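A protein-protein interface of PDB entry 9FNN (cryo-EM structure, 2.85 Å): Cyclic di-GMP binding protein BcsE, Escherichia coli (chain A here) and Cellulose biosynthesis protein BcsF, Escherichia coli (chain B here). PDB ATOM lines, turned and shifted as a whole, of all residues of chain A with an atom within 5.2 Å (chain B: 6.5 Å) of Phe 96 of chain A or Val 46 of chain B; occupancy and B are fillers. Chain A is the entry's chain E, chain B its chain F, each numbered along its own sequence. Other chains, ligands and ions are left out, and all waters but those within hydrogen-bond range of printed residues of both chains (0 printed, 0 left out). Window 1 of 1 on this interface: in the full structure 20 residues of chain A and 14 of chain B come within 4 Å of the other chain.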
ATOM      1  N   ALA A  70     -12.754   6.360 -29.364  1.00  0.00           N
ATOM      2  CA  ALA A  70     -11.409   6.709 -28.941  1.00  0.00           C
ATOM      3  C   ALA A  70     -10.595   7.144 -30.149  1.00  0.00           C
ATOM      4  O   ALA A  70     -10.883   6.766 -31.288  1.00  0.00           O
ATOM      5  CB  ALA A  70     -10.715   5.540 -28.238  1.00  0.00           C
ATOM      6  N   VAL A  71      -9.573   7.949 -29.888  1.00  0.00           N
ATOM      7  CA  VAL A  71      -8.677   8.460 -30.916  1.00  0.00           C
ATOM      8  C   VAL A  71      -7.245   8.227 -30.464  1.00  0.00           C
ATOM      9  O   VAL A  71      -6.891   8.545 -29.324  1.00  0.00           O
ATOM     10  CB  VAL A  71      -8.915   9.957 -31.195  1.00  0.00           C
ATOM     11  CG1 VAL A  71      -7.827  10.509 -32.095  1.00  0.00           C
ATOM     12  CG2 VAL A  71     -10.282  10.172 -31.816  1.00  0.00           C
ATOM     13  N   ILE A  72      -6.427   7.675 -31.352  1.00  0.00           N
ATOM     14  CA  ILE A  72      -5.013   7.448 -31.096  1.00  0.00           C
ATOM     15  C   ILE A  72      -4.221   8.257 -32.111  1.00  0.00           C
ATOM     16  O   ILE A  72      -4.461   8.150 -33.319  1.00  0.00           O
ATOM     17  CB  ILE A  72      -4.648   5.954 -31.176  1.00  0.00           C
ATOM     18  CG1 ILE A  72      -5.386   5.152 -30.103  1.00  0.00           C
ATOM     19  CG2 ILE A  72      -3.153   5.769 -31.018  1.00  0.00           C
ATOM     20  CD1 ILE A  72      -6.733   4.620 -30.529  1.00  0.00           C
ATOM     21  N   SER A  73      -3.286   9.065 -31.624  1.00  0.00           N
ATOM     22  CA  SER A  73      -2.510   9.958 -32.469  1.00  0.00           C
ATOM     23  C   SER A  73      -1.026   9.750 -32.212  1.00  0.00           C
ATOM     24  O   SER A  73      -0.622   9.172 -31.201  1.00  0.00           O
ATOM     25  CB  SER A  73      -2.885  11.425 -32.228  1.00  0.00           C
ATOM     26  OG  SER A  73      -2.111  12.288 -33.041  1.00  0.00           O
ATOM     27  N   PRO A  78      -2.561  14.978 -28.646  1.00  0.00           N
ATOM     28  CA  PRO A  78      -3.899  14.853 -29.249  1.00  0.00           C
ATOM     29  C   PRO A  78      -4.916  15.843 -28.716  1.00  0.00           C
ATOM     30  O   PRO A  78      -5.940  16.064 -29.372  1.00  0.00           O
ATOM     31  CB  PRO A  78      -4.297  13.409 -28.921  1.00  0.00           C
ATOM     32  CG  PRO A  78      -3.465  13.046 -27.742  1.00  0.00           C
ATOM     33  CD  PRO A  78      -2.165  13.764 -27.917  1.00  0.00           C
ATOM     34  N   LYS A  94     -12.261   9.642 -25.614  1.00  0.00           N
ATOM     35  CA  LYS A  94     -11.098   9.180 -24.862  1.00  0.00           C
ATOM     36  C   LYS A  94      -9.879   9.276 -25.770  1.00  0.00           C
ATOM     37  O   LYS A  94      -9.544   8.336 -26.490  1.00  0.00           O
ATOM     38  CB  LYS A  94     -11.311   7.757 -24.364  1.00  0.00           C
ATOM     39  CG  LYS A  94     -12.607   7.547 -23.604  1.00  0.00           C
ATOM     40  CD  LYS A  94     -12.434   7.816 -22.119  1.00  0.00           C
ATOM     41  CE  LYS A  94     -11.490   6.807 -21.486  1.00  0.00           C
ATOM     42  NZ  LYS A  94     -11.400   6.967 -20.009  1.00  0.00           N
ATOM     43  N   LEU A  95      -9.215  10.425 -25.739  1.00  0.00           N
ATOM     44  CA  LEU A  95      -8.011  10.603 -26.535  1.00  0.00           C
ATOM     45  C   LEU A  95      -6.882   9.729 -26.004  1.00  0.00           C
ATOM     46  O   LEU A  95      -6.789   9.451 -24.807  1.00  0.00           O
ATOM     47  CB  LEU A  95      -7.571  12.064 -26.534  1.00  0.00           C
ATOM     48  CG  LEU A  95      -8.481  13.075 -27.225  1.00  0.00           C
ATOM     49  CD1 LEU A  95      -7.911  14.472 -27.069  1.00  0.00           C
ATOM     50  CD2 LEU A  95      -8.655  12.726 -28.692  1.00  0.00           C
ATOM     51  N   PHE A  96      -6.020   9.295 -26.915  1.00  0.00           N
ATOM     52  CA  PHE A  96      -4.839   8.516 -26.586  1.00  0.00           C
ATOM     53  C   PHE A  96      -3.652   9.075 -27.353  1.00  0.00           C
ATOM     54  O   PHE A  96      -3.798   9.916 -28.242  1.00  0.00           O
ATOM     55  CB  PHE A  96      -5.035   7.032 -26.911  1.00  0.00           C
ATOM     56  CG  PHE A  96      -5.813   6.282 -25.876  1.00  0.00           C
ATOM     57  CD1 PHE A  96      -7.166   6.493 -25.722  1.00  0.00           C
ATOM     58  CD2 PHE A  96      -5.192   5.356 -25.066  1.00  0.00           C
ATOM     59  CE1 PHE A  96      -7.880   5.804 -24.773  1.00  0.00           C
ATOM     60  CE2 PHE A  96      -5.901   4.662 -24.115  1.00  0.00           C
ATOM     61  CZ  PHE A  96      -7.249   4.889 -23.969  1.00  0.00           C
ATOM     62  N   SER A  97      -2.462   8.608 -26.996  1.00  0.00           N
ATOM     63  CA  SER A  97      -1.251   9.057 -27.659  1.00  0.00           C
ATOM     64  C   SER A  97      -0.222   7.943 -27.613  1.00  0.00           C
ATOM     65  O   SER A  97      -0.191   7.148 -26.670  1.00  0.00           O
ATOM     66  CB  SER A  97      -0.693  10.329 -27.011  1.00  0.00           C
ATOM     67  OG  SER A  97       0.483  10.764 -27.671  1.00  0.00           O
ATOM     68  N   MET A  98       0.623   7.892 -28.637  1.00  0.00           N
ATOM     69  CA  MET A  98       1.630   6.849 -28.722  1.00  0.00           C
ATOM     70  C   MET A  98       2.872   7.403 -29.396  1.00  0.00           C
ATOM     71  O   MET A  98       2.831   8.432 -30.073  1.00  0.00           O
ATOM     72  CB  MET A  98       1.118   5.626 -29.492  1.00  0.00           C
ATOM     73  CG  MET A  98       0.825   5.900 -30.957  1.00  0.00           C
ATOM     74  SD  MET A  98       0.888   4.417 -31.978  1.00  0.00           S
ATOM     75  CE  MET A  98      -0.371   3.414 -31.205  1.00  0.00           C
ATOM     76  N   GLY A 104       4.354   0.844 -30.777  1.00  0.00           N
ATOM     77  CA  GLY A 104       3.069   1.363 -30.338  1.00  0.00           C
ATOM     78  C   GLY A 104       1.910   0.635 -30.986  1.00  0.00           C
ATOM     79  O   GLY A 104       0.959   0.228 -30.313  1.00  0.00           O
ATOM     80  N   LEU A 108      -0.791  -1.769 -29.146  1.00  0.00           N
ATOM     81  CA  LEU A 108      -2.078  -1.077 -29.096  1.00  0.00           C
ATOM     82  C   LEU A 108      -3.168  -1.860 -28.374  1.00  0.00           C
ATOM     83  O   LEU A 108      -3.888  -1.307 -27.538  1.00  0.00           O
ATOM     84  CB  LEU A 108      -2.518  -0.742 -30.524  1.00  0.00           C
ATOM     85  CG  LEU A 108      -3.527   0.386 -30.747  1.00  0.00           C
ATOM     86  CD1 LEU A 108      -3.369   0.946 -32.148  1.00  0.00           C
ATOM     87  CD2 LEU A 108      -4.954  -0.084 -30.537  1.00  0.00           C
ATOM     88  N   ASP A 111      -2.393  -2.150 -24.603  1.00  0.00           N
ATOM     89  CA  ASP A 111      -2.424  -0.824 -24.001  1.00  0.00           C
ATOM     90  C   ASP A 111      -3.852  -0.321 -23.847  1.00  0.00           C
ATOM     91  O   ASP A 111      -4.201   0.267 -22.818  1.00  0.00           O
ATOM     92  CB  ASP A 111      -1.592   0.148 -24.831  1.00  0.00           C
ATOM     93  CG  ASP A 111      -0.118  -0.200 -24.830  1.00  0.00           C
ATOM     94  OD1 ASP A 111       0.225  -1.324 -24.405  1.00  0.00           O
ATOM     95  OD2 ASP A 111       0.699   0.649 -25.245  1.00  0.00           O
ATOM     96  N   LEU A 112      -4.694  -0.539 -24.856  1.00  0.00           N
ATOM     97  CA  LEU A 112      -6.086  -0.127 -24.745  1.00  0.00           C
ATOM     98  C   LEU A 112      -6.849  -0.991 -23.753  1.00  0.00           C
ATOM     99  O   LEU A 112      -7.730  -0.488 -23.048  1.00  0.00           O
ATOM    100  CB  LEU A 112      -6.763  -0.169 -26.116  1.00  0.00           C
ATOM    101  CG  LEU A 112      -6.750   1.124 -26.933  1.00  0.00           C
ATOM    102  CD1 LEU A 112      -7.492   2.217 -26.189  1.00  0.00           C
ATOM    103  CD2 LEU A 112      -5.333   1.569 -27.260  1.00  0.00           C
ATOM    104  N   SER A 115      -6.393   0.258 -20.038  1.00  0.00           N
ATOM    105  CA  SER A 115      -7.038   1.485 -19.593  1.00  0.00           C
ATOM    106  C   SER A 115      -8.531   1.540 -19.880  1.00  0.00           C
ATOM    107  O   SER A 115      -9.235   2.333 -19.248  1.00  0.00           O
ATOM    108  CB  SER A 115      -6.365   2.695 -20.246  1.00  0.00           C
ATOM    109  OG  SER A 115      -4.960   2.646 -20.070  1.00  0.00           O
ATOM    110  N   ILE A 116      -9.031   0.735 -20.811  1.00  0.00           N
ATOM    111  CA  ILE A 116     -10.433   0.771 -21.210  1.00  0.00           C
ATOM    112  C   ILE A 116     -10.922  -0.656 -21.408  1.00  0.00           C
ATOM    113  O   ILE A 116     -10.169  -1.523 -21.863  1.00  0.00           O
ATOM    114  CB  ILE A 116     -10.634   1.595 -22.502  1.00  0.00           C
ATOM    115  CG1 ILE A 116     -10.265   3.061 -22.285  1.00  0.00           C
ATOM    116  CG2 ILE A 116     -12.069   1.501 -23.003  1.00  0.00           C
ATOM    117  CD1 ILE A 116     -10.589   3.936 -23.473  1.00  0.00           C
ATOM    118  N   PRO B  43       0.443   0.517 -19.291  1.00  0.00           N
ATOM    119  CA  PRO B  43       0.411   0.980 -20.664  1.00  0.00           C
ATOM    120  C   PRO B  43       1.868   1.271 -21.017  1.00  0.00           C
ATOM    121  O   PRO B  43       2.396   2.223 -20.498  1.00  0.00           O
ATOM    122  CB  PRO B  43      -0.436   2.250 -20.581  1.00  0.00           C
ATOM    123  CG  PRO B  43      -0.832   2.403 -19.131  1.00  0.00           C
ATOM    124  CD  PRO B  43       0.170   1.590 -18.344  1.00  0.00           C
ATOM    125  N   ARG B  44       2.509   0.452 -21.849  1.00  0.00           N
ATOM    126  CA  ARG B  44       3.928   0.656 -22.111  1.00  0.00           C
ATOM    127  C   ARG B  44       4.194   1.754 -23.132  1.00  0.00           C
ATOM    128  O   ARG B  44       5.168   2.501 -22.992  1.00  0.00           O
ATOM    129  CB  ARG B  44       4.574  -0.652 -22.577  1.00  0.00           C
ATOM    130  CG  ARG B  44       6.086  -0.569 -22.722  1.00  0.00           C
ATOM    131  CD  ARG B  44       6.695  -1.928 -23.017  1.00  0.00           C
ATOM    132  NE  ARG B  44       8.143  -1.850 -23.173  1.00  0.00           N
ATOM    133  CZ  ARG B  44       8.924  -2.884 -23.450  1.00  0.00           C
ATOM    134  NH1 ARG B  44       8.430  -4.100 -23.613  1.00  0.00           N
ATOM    135  NH2 ARG B  44      10.235  -2.694 -23.570  1.00  0.00           N
ATOM    136  N   TYR B  45       3.356   1.876 -24.162  1.00  0.00           N
ATOM    137  CA  TYR B  45       3.629   2.846 -25.217  1.00  0.00           C
ATOM    138  C   TYR B  45       2.459   3.788 -25.476  1.00  0.00           C
ATOM    139  O   TYR B  45       2.670   4.956 -25.815  1.00  0.00           O
ATOM    140  CB  TYR B  45       4.018   2.126 -26.505  1.00  0.00           C
ATOM    141  CG  TYR B  45       5.355   1.432 -26.423  1.00  0.00           C
ATOM    142  CD1 TYR B  45       6.535   2.157 -26.433  1.00  0.00           C
ATOM    143  CD2 TYR B  45       5.436   0.050 -26.341  1.00  0.00           C
ATOM    144  CE1 TYR B  45       7.760   1.530 -26.362  1.00  0.00           C
ATOM    145  CE2 TYR B  45       6.656  -0.587 -26.271  1.00  0.00           C
ATOM    146  CZ  TYR B  45       7.814   0.158 -26.280  1.00  0.00           C
ATOM    147  OH  TYR B  45       9.034  -0.471 -26.209  1.00  0.00           O
ATOM    148  N   VAL B  46       1.231   3.303 -25.330  1.00  0.00           N
ATOM    149  CA  VAL B  46       0.041   4.115 -25.558  1.00  0.00           C
ATOM    150  C   VAL B  46      -0.461   4.610 -24.208  1.00  0.00           C
ATOM    151  O   VAL B  46      -0.994   3.834 -23.410  1.00  0.00           O
ATOM    152  CB  VAL B  46      -1.044   3.331 -26.303  1.00  0.00           C
ATOM    153  CG1 VAL B  46      -2.269   4.195 -26.513  1.00  0.00           C
ATOM    154  CG2 VAL B  46      -0.507   2.831 -27.630  1.00  0.00           C
ATOM    155  N   LYS B  47      -0.298   5.910 -23.954  1.00  0.00           N
ATOM    156  CA  LYS B  47      -0.692   6.522 -22.692  1.00  0.00           C
ATOM    157  C   LYS B  47      -1.900   7.415 -22.916  1.00  0.00           C
ATOM    158  O   LYS B  47      -1.814   8.356 -23.719  1.00  0.00           O
ATOM    159  CB  LYS B  47       0.461   7.334 -22.112  1.00  0.00           C
ATOM    160  CG  LYS B  47       1.832   6.744 -22.370  1.00  0.00           C
ATOM    161  CD  LYS B  47       2.054   5.474 -21.576  1.00  0.00           C
ATOM    162  CE  LYS B  47       3.449   4.929 -21.816  1.00  0.00           C
ATOM    163  NZ  LYS B  47       4.498   5.933 -21.497  1.00  0.00           N
ATOM    164  N   PRO B  48      -3.035   7.172 -22.250  1.00  0.00           N
ATOM    165  CA  PRO B  48      -4.206   8.041 -22.445  1.00  0.00           C
ATOM    166  C   PRO B  48      -3.928   9.494 -22.096  1.00  0.00           C
ATOM    167  O   PRO B  48      -3.667   9.826 -20.936  1.00  0.00           O
ATOM    168  CB  PRO B  48      -5.259   7.431 -21.507  1.00  0.00           C
ATOM    169  CG  PRO B  48      -4.494   6.579 -20.556  1.00  0.00           C
ATOM    170  CD  PRO B  48      -3.310   6.075 -21.311  1.00  0.00           C
ATOM    171  N   ALA B  49      -3.977  10.366 -23.106  1.00  0.00           N
ATOM    172  CA  ALA B  49      -3.724  11.784 -22.877  1.00  0.00           C
ATOM    173  C   ALA B  49      -4.797  12.405 -21.996  1.00  0.00           C
ATOM    174  O   ALA B  49      -4.486  13.182 -21.085  1.00  0.00           O
ATOM    175  CB  ALA B  49      -3.631  12.522 -24.209  1.00  0.00           C
ATOM    176  N   GLY B  50      -6.063  12.081 -22.246  1.00  0.00           N
ATOM    177  CA  GLY B  50      -7.126  12.590 -21.405  1.00  0.00           C
ATOM    178  C   GLY B  50      -8.466  12.726 -22.091  1.00  0.00           C
ATOM    179  O   GLY B  50      -8.544  13.174 -23.239  1.00  0.00           O
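Printed residues of chain B that touch a printed residue of chain A: Arg 44, Tyr 45, Val 46, Lys 47, Pro 48, Ala 49 and Gly 50.
Hydrophobic or aromatic side chains of chain B within 4 Å of the printed part of chain A: Tyr 45, Val 46, Pro 48 and Ala 49.
Of the 16 printed residues of chain A, 7 touch a printed residue of chain B.
Printed residues of chain A that touch a printed residue of chain B: Pro 78, Leu 95, Phe 96, Ser 97, Met 98, Asp 111 and Ser 115.
Among the printed residues, no Asp or Glu carboxylate lies within 4 Å of a Lys or Arg side-chain nitrogen of the other chain.
The backbone NH (N) of Ala 49 of chain B is in hydrogen-bond range of the backbone carbonyl oxygen (O) of Leu 95 of chain A.
The backbone carbonyl oxygen of Ser 97 of chain A lies within hydrogen-bond range of the backbone NH of Lys 47 of chain B (3.0 Å).
The side-chain carboxylate (OD2) of Asp 111 of chain A sits at hydrogen-bond distance from the backbone NH (N) of Tyr 45 of chain B (3.1 Å).
The backbone NH (N) of Val 46 of chain B sits at hydrogen-bond distance from the side-chain carboxylate (OD2) of Asp 111 of chain A.
CG of Pro 78 of chain A touches CB of Ala 49 of chain B, at 3.6 Å.
Gly 50 of chain B touches Leu 95 of chain A (O to CB, 3.6 Å).
Phe 96 of chain A touches Val 46 of chain B.
Phe 96 of chain A touches Pro 48 of chain B (CE2 to CB, 3.9 Å).
Tyr 45 of chain B touches Ser 97 of chain A (O to O, 3.7 Å).
Ser 97 of chain A touches Val 46 of chain B (O to CA, 3.2 Å).
Met 98 of chain A touches Tyr 45 of chain B.
CG2 of Val 46 of chain B touches CE of Met 98 of chain A (3.6 Å).
Arg 44 of chain B touches Asp 111 of chain A.
OG of Ser 115 of chain A touches CG of Pro 48 of chain B, 3.99 Å away.
The backbone carbonyl oxygen (O) of Val 71 of chain A lies within hydrogen-bond range of the backbone NH (N) of Phe 96 of chain A (2.7 Å).
The backbone NH (N) of Met 98 of chain A is in hydrogen-bond range of the backbone carbonyl oxygen (O) of Ser 73 of chain A (3.1 Å).
The side-chain hydroxyl of Tyr 45 of chain B sits at hydrogen-bond distance from the guanidinium group of Arg 44 of chain B (3.5 Å).
Phe 96 of chain A touches just these residues of chain B: Val 46 and Pro 48.
Of the printed residues of chain B, Ser 115 of chain A touches Pro 48.
Of the printed residues of chain A, Tyr 45 of chain B touches Ser 97 (3.7 Å), Met 98 (3.6 Å) and Asp 111 (3.1 Å).
Of the printed residues of chain A, Val 46 of chain B touches Phe 96, Ser 97, Met 98 and Asp 111.
The nearest residue of chain B that does not touch Phe 96 of chain A is Ala 49 of chain B (4.03 Å).
The nearest printed residue of chain A that does not touch Val 46 of chain B is Gly 104 of chain A (4.02 Å).
The nearest printed residue of chain B that does not touch Ser 115 of chain A is Pro 43 of chain B (4.2 Å).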
